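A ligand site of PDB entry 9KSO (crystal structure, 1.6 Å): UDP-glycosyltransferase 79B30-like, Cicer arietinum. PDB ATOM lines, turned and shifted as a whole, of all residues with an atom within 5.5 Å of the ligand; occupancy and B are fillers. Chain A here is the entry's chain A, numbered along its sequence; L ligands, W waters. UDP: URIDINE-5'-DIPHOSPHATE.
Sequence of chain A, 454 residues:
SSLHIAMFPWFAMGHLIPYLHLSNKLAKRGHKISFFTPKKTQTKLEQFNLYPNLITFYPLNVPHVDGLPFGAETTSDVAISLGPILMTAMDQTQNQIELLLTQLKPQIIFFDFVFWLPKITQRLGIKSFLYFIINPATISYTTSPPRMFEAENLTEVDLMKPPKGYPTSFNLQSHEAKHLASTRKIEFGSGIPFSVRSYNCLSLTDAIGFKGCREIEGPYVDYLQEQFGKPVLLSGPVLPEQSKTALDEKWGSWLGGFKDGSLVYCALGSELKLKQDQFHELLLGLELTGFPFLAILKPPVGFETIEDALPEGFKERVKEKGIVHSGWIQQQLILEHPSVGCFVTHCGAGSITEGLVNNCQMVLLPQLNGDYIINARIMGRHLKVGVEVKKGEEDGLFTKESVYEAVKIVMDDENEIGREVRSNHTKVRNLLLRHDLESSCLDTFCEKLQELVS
Residues that only touch the ligand: Gly 14 (3.6 Å), Ile 17 (3.8 Å), Gly 269 (3.2 Å), Glu 271 (3.6 Å), Trp 328 (3.3 Å) and Gly 348 (3.6 Å).
Hydrophobic or aromatic side chains that line the ligand: Ile 17, Trp 328, Ile 329, His 346 and Tyr 372.
15 residues have an atom within 4 Å of the ligand: Gly 14, Ile 17, Gly 269, Ser 270, Glu 271, Trp 328, Ile 329, Gln 331, His 346, Gly 348, Ala 349, Gly 350, Ser 351, Glu 354 and Tyr 372.
The nearest printed residue that does not touch the ligand is Gly 327 (4.1 Å).
OE1 of Glu 354 sits at hydrogen-bond distance from O2' of the ligand (2.6 Å).
An oxygen (O2A) of the ligand sits at hydrogen-bond distance from the backbone NH (N) of Ser 351.
O2A of the ligand lies within hydrogen-bond range of OG of Ser 351.
The backbone NH (N) of Ile 329 is in hydrogen-bond range of an oxygen (O4) of the ligand (3.1 Å).
N3 of the ligand lies within hydrogen-bond range of O of Ile 329 (2.7 Å).
An oxygen (O3B) of the ligand sits at hydrogen-bond distance from the backbone NH (N) of Ser 270 (2.8 Å).
An oxygen (O3B) of the ligand is in hydrogen-bond range of the side-chain hydroxyl (OG) of Ser 270, 3.3 Å away.
An oxygen (O2B) of the ligand is in hydrogen-bond range of the side-chain hydroxyl (OH) of Tyr 372, at 2.9 Å.
A ring nitrogen (NE2) of His 346 sits at hydrogen-bond distance from an oxygen (O2B) of the ligand (3.0 Å).
An oxygen (O1A) of the ligand sits at hydrogen-bond distance from the backbone NH of Gly 350, 3.1 Å away.
NE2 of Gln 331 lies within hydrogen-bond range of O2' of the ligand, 3.4 Å away.
The backbone NH (N) of Ala 349 is in hydrogen-bond range of an oxygen (O1A) of the ligand, at 3.4 Å.
OE1 of Glu 354 sits at hydrogen-bond distance from NE2 of Gln 331 (3.0 Å).
OG of Ser 351 is in hydrogen-bond range of NE2 of Gln 331 (3.0 Å).
The side-chain carboxylate of Glu 271 lies within hydrogen-bond range of the side-chain hydroxyl of Tyr 372.
OH of Tyr 265 is in hydrogen-bond range of OE1 of Gln 331, at 2.8 Å.
Water W1 lies within hydrogen-bond range of O1B of the ligand (2.4 Å), N of Gly 14 (2.8 Å), OE2 of Glu 271 (3.3 Å) and N of Met 13 (3.5 Å).
Water W5 lies within hydrogen-bond range of an oxygen (O2B) of the ligand (2.6 Å), the backbone carbonyl oxygen (O) of Leu 268 (2.8 Å), the backbone NH (N) of Glu 271 (2.9 Å) and the backbone NH (N) of Ser 270 (3.3 Å).
Water W4 bridges O1B of the ligand (2.7 Å) and OE2 of Glu 271 (3.2 Å).
Water W2 lies within hydrogen-bond range of the backbone carbonyl oxygen (O) of Gly 14 (2.6 Å), an oxygen (O1A) of the ligand (2.9 Å) and the backbone NH (N) of Gly 350 (3.2 Å).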
ATOM      1  N   MET A  13     -32.564  -7.296 -35.191  1.00  0.00           N
ATOM      2  CA  MET A  13     -31.505  -8.292 -35.286  1.00  0.00           C
ATOM      3  C   MET A  13     -31.629  -9.344 -34.186  1.00  0.00           C
ATOM      4  O   MET A  13     -31.345 -10.523 -34.415  1.00  0.00           O
ATOM      5  CB  MET A  13     -30.139  -7.595 -35.274  1.00  0.00           C
ATOM      6  CG  MET A  13     -29.812  -6.730 -36.525  1.00  0.00           C
ATOM      7  SD  MET A  13     -30.070  -7.598 -38.093  1.00  0.00           S
ATOM      8  CE  MET A  13     -28.500  -8.478 -38.181  1.00  0.00           C
ATOM      9  N   GLY A  14     -32.123  -8.944 -33.006  1.00  0.00           N
ATOM     10  CA  GLY A  14     -32.356  -9.861 -31.894  1.00  0.00           C
ATOM     11  C   GLY A  14     -33.470 -10.854 -32.133  1.00  0.00           C
ATOM     12  O   GLY A  14     -33.602 -11.816 -31.368  1.00  0.00           O
ATOM     13  N   ILE A  17     -31.804 -13.043 -35.895  1.00  0.00           N
ATOM     14  CA  ILE A  17     -30.664 -13.930 -35.691  1.00  0.00           C
ATOM     15  C   ILE A  17     -31.112 -15.249 -35.048  1.00  0.00           C
ATOM     16  O   ILE A  17     -30.776 -16.313 -35.586  1.00  0.00           O
ATOM     17  CB  ILE A  17     -29.562 -13.248 -34.867  1.00  0.00           C
ATOM     18  CG1 ILE A  17     -28.822 -12.217 -35.734  1.00  0.00           C
ATOM     19  CG2 ILE A  17     -28.597 -14.286 -34.331  1.00  0.00           C
ATOM     20  CD1 ILE A  17     -27.877 -11.316 -34.938  1.00  0.00           C
ATOM     21  N   TYR A 265     -15.434  -7.555 -21.799  1.00  0.00           N
ATOM     22  CA  TYR A 265     -16.228  -7.195 -22.968  1.00  0.00           C
ATOM     23  C   TYR A 265     -17.554  -6.609 -22.501  1.00  0.00           C
ATOM     24  O   TYR A 265     -18.254  -7.236 -21.700  1.00  0.00           O
ATOM     25  CB  TYR A 265     -16.464  -8.422 -23.864  1.00  0.00           C
ATOM     26  CG  TYR A 265     -17.385  -8.187 -25.030  1.00  0.00           C
ATOM     27  CD1 TYR A 265     -16.960  -7.488 -26.173  1.00  0.00           C
ATOM     28  CD2 TYR A 265     -18.682  -8.681 -25.022  1.00  0.00           C
ATOM     29  CE1 TYR A 265     -17.820  -7.266 -27.239  1.00  0.00           C
ATOM     30  CE2 TYR A 265     -19.550  -8.470 -26.082  1.00  0.00           C
ATOM     31  CZ  TYR A 265     -19.099  -7.766 -27.198  1.00  0.00           C
ATOM     32  OH  TYR A 265     -19.970  -7.578 -28.252  1.00  0.00           O
ATOM     33  N   LEU A 268     -24.268  -3.520 -25.169  1.00  0.00           N
ATOM     34  CA  LEU A 268     -25.675  -3.331 -24.826  1.00  0.00           C
ATOM     35  C   LEU A 268     -26.576  -3.539 -26.036  1.00  0.00           C
ATOM     36  O   LEU A 268     -27.587  -2.851 -26.218  1.00  0.00           O
ATOM     37  CB  LEU A 268     -25.875  -1.935 -24.204  1.00  0.00           C
ATOM     38  CG  LEU A 268     -24.896  -1.606 -23.072  1.00  0.00           C
ATOM     39  CD1 LEU A 268     -25.173  -0.187 -22.538  1.00  0.00           C
ATOM     40  CD2 LEU A 268     -24.926  -2.635 -21.937  1.00  0.00           C
ATOM     41  N   GLY A 269     -26.243  -4.486 -26.885  1.00  0.00           N
ATOM     42  CA  GLY A 269     -27.134  -4.773 -27.991  1.00  0.00           C
ATOM     43  C   GLY A 269     -27.033  -3.722 -29.089  1.00  0.00           C
ATOM     44  O   GLY A 269     -26.156  -2.878 -29.109  1.00  0.00           O
ATOM     45  N   SER A 270     -28.003  -3.778 -29.996  1.00  0.00           N
ATOM     46  CA  SER A 270     -27.960  -2.923 -31.177  1.00  0.00           C
ATOM     47  C   SER A 270     -29.123  -1.934 -31.250  1.00  0.00           C
ATOM     48  O   SER A 270     -29.272  -1.276 -32.297  1.00  0.00           O
ATOM     49  CB  SER A 270     -27.946  -3.777 -32.449  1.00  0.00           C
ATOM     50  OG  SER A 270     -29.131  -4.550 -32.553  1.00  0.00           O
ATOM     51  N   GLU A 271     -29.932  -1.801 -30.208  1.00  0.00           N
ATOM     52  CA  GLU A 271     -31.137  -0.977 -30.245  1.00  0.00           C
ATOM     53  C   GLU A 271     -31.095   0.232 -29.324  1.00  0.00           C
ATOM     54  O   GLU A 271     -32.034   1.050 -29.362  1.00  0.00           O
ATOM     55  CB  GLU A 271     -32.380  -1.799 -29.876  1.00  0.00           C
ATOM     56  CG  GLU A 271     -32.619  -3.042 -30.679  1.00  0.00           C
ATOM     57  CD  GLU A 271     -33.859  -3.793 -30.194  1.00  0.00           C
ATOM     58  OE1 GLU A 271     -33.967  -4.009 -28.965  1.00  0.00           O
ATOM     59  OE2 GLU A 271     -34.718  -4.173 -31.025  1.00  0.00           O
ATOM     60  N   LEU A 272     -30.076   0.362 -28.479  1.00  0.00           N
ATOM     61  CA  LEU A 272     -30.116   1.320 -27.379  1.00  0.00           C
ATOM     62  C   LEU A 272     -28.965   2.301 -27.451  1.00  0.00           C
ATOM     63  O   LEU A 272     -27.856   1.962 -27.871  1.00  0.00           O
ATOM     64  CB  LEU A 272     -30.038   0.641 -26.007  1.00  0.00           C
ATOM     65  CG  LEU A 272     -30.800  -0.647 -25.750  1.00  0.00           C
ATOM     66  CD1 LEU A 272     -30.300  -1.226 -24.441  1.00  0.00           C
ATOM     67  CD2 LEU A 272     -32.300  -0.397 -25.702  1.00  0.00           C
ATOM     68  N   ILE A 296     -18.644  -1.983 -26.720  1.00  0.00           N
ATOM     69  CA  ILE A 296     -19.370  -1.803 -27.975  1.00  0.00           C
ATOM     70  C   ILE A 296     -20.623  -1.003 -27.638  1.00  0.00           C
ATOM     71  O   ILE A 296     -21.616  -1.547 -27.153  1.00  0.00           O
ATOM     72  CB  ILE A 296     -19.720  -3.150 -28.627  1.00  0.00           C
ATOM     73  CG1 ILE A 296     -18.487  -4.055 -28.678  1.00  0.00           C
ATOM     74  CG2 ILE A 296     -20.376  -2.947 -30.004  1.00  0.00           C
ATOM     75  CD1 ILE A 296     -17.317  -3.462 -29.466  1.00  0.00           C
ATOM     76  N   GLY A 327     -19.530   0.383 -33.963  1.00  0.00           N
ATOM     77  CA  GLY A 327     -19.989  -0.402 -35.098  1.00  0.00           C
ATOM     78  C   GLY A 327     -20.471  -1.808 -34.701  1.00  0.00           C
ATOM     79  O   GLY A 327     -20.166  -2.298 -33.621  1.00  0.00           O
ATOM     80  N   TRP A 328     -21.246  -2.419 -35.600  1.00  0.00           N
ATOM     81  CA  TRP A 328     -21.635  -3.818 -35.451  1.00  0.00           C
ATOM     82  C   TRP A 328     -20.411  -4.716 -35.468  1.00  0.00           C
ATOM     83  O   TRP A 328     -19.618  -4.672 -36.405  1.00  0.00           O
ATOM     84  CB  TRP A 328     -22.565  -4.206 -36.601  1.00  0.00           C
ATOM     85  CG  TRP A 328     -23.019  -5.632 -36.560  1.00  0.00           C
ATOM     86  CD1 TRP A 328     -22.396  -6.725 -37.108  1.00  0.00           C
ATOM     87  CD2 TRP A 328     -24.187  -6.116 -35.931  1.00  0.00           C
ATOM     88  NE1 TRP A 328     -23.122  -7.872 -36.866  1.00  0.00           N
ATOM     89  CE2 TRP A 328     -24.238  -7.517 -36.136  1.00  0.00           C
ATOM     90  CE3 TRP A 328     -25.222  -5.506 -35.229  1.00  0.00           C
ATOM     91  CZ2 TRP A 328     -25.276  -8.307 -35.659  1.00  0.00           C
ATOM     92  CZ3 TRP A 328     -26.250  -6.298 -34.742  1.00  0.00           C
ATOM     93  CH2 TRP A 328     -26.275  -7.675 -34.957  1.00  0.00           C
ATOM     94  N   ILE A 329     -20.243  -5.550 -34.444  1.00  0.00           N
ATOM     95  CA  ILE A 329     -19.143  -6.508 -34.443  1.00  0.00           C
ATOM     96  C   ILE A 329     -19.692  -7.936 -34.364  1.00  0.00           C
ATOM     97  O   ILE A 329     -20.883  -8.143 -34.197  1.00  0.00           O
ATOM     98  CB  ILE A 329     -18.110  -6.221 -33.329  1.00  0.00           C
ATOM     99  CG1 ILE A 329     -18.768  -5.774 -32.032  1.00  0.00           C
ATOM    100  CG2 ILE A 329     -17.137  -5.136 -33.793  1.00  0.00           C
ATOM    101  CD1 ILE A 329     -19.579  -6.825 -31.361  1.00  0.00           C
ATOM    102  N   GLN A 330     -18.805  -8.921 -34.546  1.00  0.00           N
ATOM    103  CA  GLN A 330     -19.200 -10.328 -34.456  1.00  0.00           C
ATOM    104  C   GLN A 330     -19.176 -10.754 -32.989  1.00  0.00           C
ATOM    105  O   GLN A 330     -18.227 -11.394 -32.501  1.00  0.00           O
ATOM    106  CB  GLN A 330     -18.302 -11.201 -35.316  1.00  0.00           C
ATOM    107  CG  GLN A 330     -18.193 -10.707 -36.756  1.00  0.00           C
ATOM    108  CD  GLN A 330     -16.948 -11.245 -37.449  1.00  0.00           C
ATOM    109  OE1 GLN A 330     -15.879 -10.651 -37.341  1.00  0.00           O
ATOM    110  NE2 GLN A 330     -17.092 -12.347 -38.183  1.00  0.00           N
ATOM    111  N   GLN A 331     -20.233 -10.384 -32.254  1.00  0.00           N
ATOM    112  CA  GLN A 331     -20.240 -10.582 -30.808  1.00  0.00           C
ATOM    113  C   GLN A 331     -20.049 -12.040 -30.442  1.00  0.00           C
ATOM    114  O   GLN A 331     -19.304 -12.353 -29.493  1.00  0.00           O
ATOM    115  CB  GLN A 331     -21.548 -10.066 -30.193  1.00  0.00           C
ATOM    116  CG  GLN A 331     -21.655 -10.430 -28.746  1.00  0.00           C
ATOM    117  CD  GLN A 331     -22.756  -9.655 -28.038  1.00  0.00           C
ATOM    118  OE1 GLN A 331     -22.637  -8.442 -27.860  1.00  0.00           O
ATOM    119  NE2 GLN A 331     -23.812 -10.361 -27.579  1.00  0.00           N
ATOM    120  N   GLN A 332     -20.713 -12.956 -31.142  1.00  0.00           N
ATOM    121  CA  GLN A 332     -20.627 -14.364 -30.783  1.00  0.00           C
ATOM    122  C   GLN A 332     -19.181 -14.856 -30.849  1.00  0.00           C
ATOM    123  O   GLN A 332     -18.729 -15.587 -29.961  1.00  0.00           O
ATOM    124  CB  GLN A 332     -21.546 -15.189 -31.690  1.00  0.00           C
ATOM    125  CG  GLN A 332     -21.306 -16.669 -31.617  1.00  0.00           C
ATOM    126  CD  GLN A 332     -22.095 -17.431 -32.633  1.00  0.00           C
ATOM    127  OE1 GLN A 332     -23.097 -16.931 -33.182  1.00  0.00           O
ATOM    128  NE2 GLN A 332     -21.651 -18.647 -32.930  1.00  0.00           N
ATOM    129  N   HIS A 346     -26.366  -5.998 -21.336  1.00  0.00           N
ATOM    130  CA  HIS A 346     -27.688  -5.407 -21.107  1.00  0.00           C
ATOM    131  C   HIS A 346     -28.773  -6.448 -20.870  1.00  0.00           C
ATOM    132  O   HIS A 346     -29.924  -6.066 -20.647  1.00  0.00           O
ATOM    133  CB  HIS A 346     -28.073  -4.524 -22.286  1.00  0.00           C
ATOM    134  CG  HIS A 346     -28.470  -5.285 -23.501  1.00  0.00           C
ATOM    135  ND1 HIS A 346     -27.703  -6.301 -24.041  1.00  0.00           N
ATOM    136  CD2 HIS A 346     -29.558  -5.180 -24.304  1.00  0.00           C
ATOM    137  CE1 HIS A 346     -28.298  -6.776 -25.112  1.00  0.00           C
ATOM    138  NE2 HIS A 346     -29.420  -6.114 -25.289  1.00  0.00           N
ATOM    139  N   GLY A 348     -30.110  -8.677 -22.885  1.00  0.00           N
ATOM    140  CA  GLY A 348     -30.908  -9.164 -24.006  1.00  0.00           C
ATOM    141  C   GLY A 348     -30.887 -10.679 -24.080  1.00  0.00           C
ATOM    142  O   GLY A 348     -29.892 -11.322 -23.749  1.00  0.00           O
ATOM    143  N   ALA A 349     -32.008 -11.260 -24.532  1.00  0.00           N
ATOM    144  CA  ALA A 349     -32.158 -12.718 -24.520  1.00  0.00           C
ATOM    145  C   ALA A 349     -31.086 -13.416 -25.344  1.00  0.00           C
ATOM    146  O   ALA A 349     -30.625 -14.500 -24.979  1.00  0.00           O
ATOM    147  CB  ALA A 349     -33.547 -13.095 -25.023  1.00  0.00           C
ATOM    148  N   GLY A 350     -30.674 -12.827 -26.474  1.00  0.00           N
ATOM    149  CA  GLY A 350     -29.657 -13.469 -27.295  1.00  0.00           C
ATOM    150  C   GLY A 350     -28.282 -13.375 -26.663  1.00  0.00           C
ATOM    151  O   GLY A 350     -27.526 -14.355 -26.649  1.00  0.00           O
ATOM    152  N   SER A 351     -27.937 -12.200 -26.133  1.00  0.00           N
ATOM    153  CA  SER A 351     -26.664 -12.011 -25.459  1.00  0.00           C
ATOM    154  C   SER A 351     -26.552 -12.895 -24.230  1.00  0.00           C
ATOM    155  O   SER A 351     -25.465 -13.376 -23.916  1.00  0.00           O
ATOM    156  CB  SER A 351     -26.485 -10.545 -25.053  1.00  0.00           C
ATOM    157  OG  SER A 351     -26.336  -9.706 -26.182  1.00  0.00           O
ATOM    158  N   ILE A 352     -27.678 -13.114 -23.521  1.00  0.00           N
ATOM    159  CA  ILE A 352     -27.660 -14.001 -22.363  1.00  0.00           C
ATOM    160  C   ILE A 352     -27.253 -15.415 -22.789  1.00  0.00           C
ATOM    161  O   ILE A 352     -26.373 -16.038 -22.158  1.00  0.00           O
ATOM    162  CB  ILE A 352     -29.034 -14.003 -21.658  1.00  0.00           C
ATOM    163  CG1 ILE A 352     -29.270 -12.720 -20.862  1.00  0.00           C
ATOM    164  CG2 ILE A 352     -29.119 -15.195 -20.686  1.00  0.00           C
ATOM    165  CD1 ILE A 352     -28.245 -12.477 -19.785  1.00  0.00           C
ATOM    166  N   GLU A 354     -25.562 -16.310 -25.447  1.00  0.00           N
ATOM    167  CA  GLU A 354     -24.182 -16.292 -25.898  1.00  0.00           C
ATOM    168  C   GLU A 354     -23.206 -16.249 -24.736  1.00  0.00           C
ATOM    169  O   GLU A 354     -22.135 -16.875 -24.801  1.00  0.00           O
ATOM    170  CB  GLU A 354     -23.974 -15.113 -26.857  1.00  0.00           C
ATOM    171  CG  GLU A 354     -24.756 -15.358 -28.143  1.00  0.00           C
ATOM    172  CD  GLU A 354     -25.042 -14.118 -28.955  1.00  0.00           C
ATOM    173  OE1 GLU A 354     -24.487 -13.043 -28.662  1.00  0.00           O
ATOM    174  OE2 GLU A 354     -25.857 -14.240 -29.902  1.00  0.00           O
ATOM    175  N   TYR A 372     -35.208  -7.472 -20.390  1.00  0.00           N
ATOM    176  CA  TYR A 372     -33.854  -7.356 -19.857  1.00  0.00           C
ATOM    177  C   TYR A 372     -33.877  -7.446 -18.329  1.00  0.00           C
ATOM    178  O   TYR A 372     -33.039  -8.124 -17.713  1.00  0.00           O
ATOM    179  CB  TYR A 372     -33.191  -6.042 -20.265  1.00  0.00           C
ATOM    180  CG  TYR A 372     -33.146  -5.721 -21.754  1.00  0.00           C
ATOM    181  CD1 TYR A 372     -33.314  -6.700 -22.710  1.00  0.00           C
ATOM    182  CD2 TYR A 372     -32.897  -4.435 -22.171  1.00  0.00           C
ATOM    183  CE1 TYR A 372     -33.261  -6.380 -24.081  1.00  0.00           C
ATOM    184  CE2 TYR A 372     -32.833  -4.102 -23.518  1.00  0.00           C
ATOM    185  CZ  TYR A 372     -33.022  -5.088 -24.464  1.00  0.00           C
ATOM    186  OH  TYR A 372     -32.974  -4.751 -25.793  1.00  0.00           O
HETATM  187  N1  UDP L   1     -24.974  -8.544 -31.964  1.00  0.00           N
HETATM  188  C2  UDP L   1     -23.849  -8.673 -32.751  1.00  0.00           C
HETATM  189  N3  UDP L   1     -23.087  -7.529 -32.841  1.00  0.00           N
HETATM  190  C4  UDP L   1     -23.350  -6.306 -32.267  1.00  0.00           C
HETATM  191  C5  UDP L   1     -24.556  -6.247 -31.490  1.00  0.00           C
HETATM  192  C6  UDP L   1     -25.317  -7.349 -31.379  1.00  0.00           C
HETATM  193  O2  UDP L   1     -23.518  -9.724 -33.289  1.00  0.00           O
HETATM  194  O4  UDP L   1     -22.562  -5.373 -32.452  1.00  0.00           O
HETATM  195  C1' UDP L   1     -25.871  -9.707 -31.874  1.00  0.00           C
HETATM  196  C2' UDP L   1     -25.757 -10.477 -30.559  1.00  0.00           C
HETATM  197  O2' UDP L   1     -24.701 -11.420 -30.633  1.00  0.00           O
HETATM  198  C3' UDP L   1     -27.156 -11.104 -30.492  1.00  0.00           C
HETATM  199  C4' UDP L   1     -28.046  -9.987 -31.063  1.00  0.00           C
HETATM  200  O4' UDP L   1     -27.181  -9.196 -31.917  1.00  0.00           O
HETATM  201  O3' UDP L   1     -27.223 -12.308 -31.244  1.00  0.00           O
HETATM  202  C5' UDP L   1     -28.610  -9.050 -30.032  1.00  0.00           C
HETATM  203  O5' UDP L   1     -29.718  -9.703 -29.425  1.00  0.00           O
HETATM  204  PA  UDP L   1     -30.039  -9.404 -27.890  1.00  0.00           P
HETATM  205  O1A UDP L   1     -31.349 -10.047 -27.594  1.00  0.00           O
HETATM  206  O2A UDP L   1     -28.849  -9.740 -27.035  1.00  0.00           O
HETATM  207  O3A UDP L   1     -30.124  -7.806 -27.881  1.00  0.00           O
HETATM  208  PB  UDP L   1     -30.628  -6.542 -28.790  1.00  0.00           P
HETATM  209  O1B UDP L   1     -31.853  -7.031 -29.547  1.00  0.00           O
HETATM  210  O2B UDP L   1     -30.955  -5.492 -27.745  1.00  0.00           O
HETATM  211  O3B UDP L   1     -29.494  -6.125 -29.701  1.00  0.00           O
HETATM  212  O   HOH W   1     -32.505  -6.476 -31.807  1.00  0.00           O
HETATM  213  O   HOH W   2     -31.966 -12.324 -29.347  1.00  0.00           O
HETATM  214  O   HOH W   3     -29.702 -13.519 -30.782  1.00  0.00           O
HETATM  215  O   HOH W   4     -34.581  -7.174 -29.852  1.00  0.00           O
HETATM  216  O   HOH W   5     -30.040  -3.018 -27.571  1.00  0.00           O
HETATM  217  O   HOH W   6     -24.583 -13.239 -33.193  1.00  0.00           O
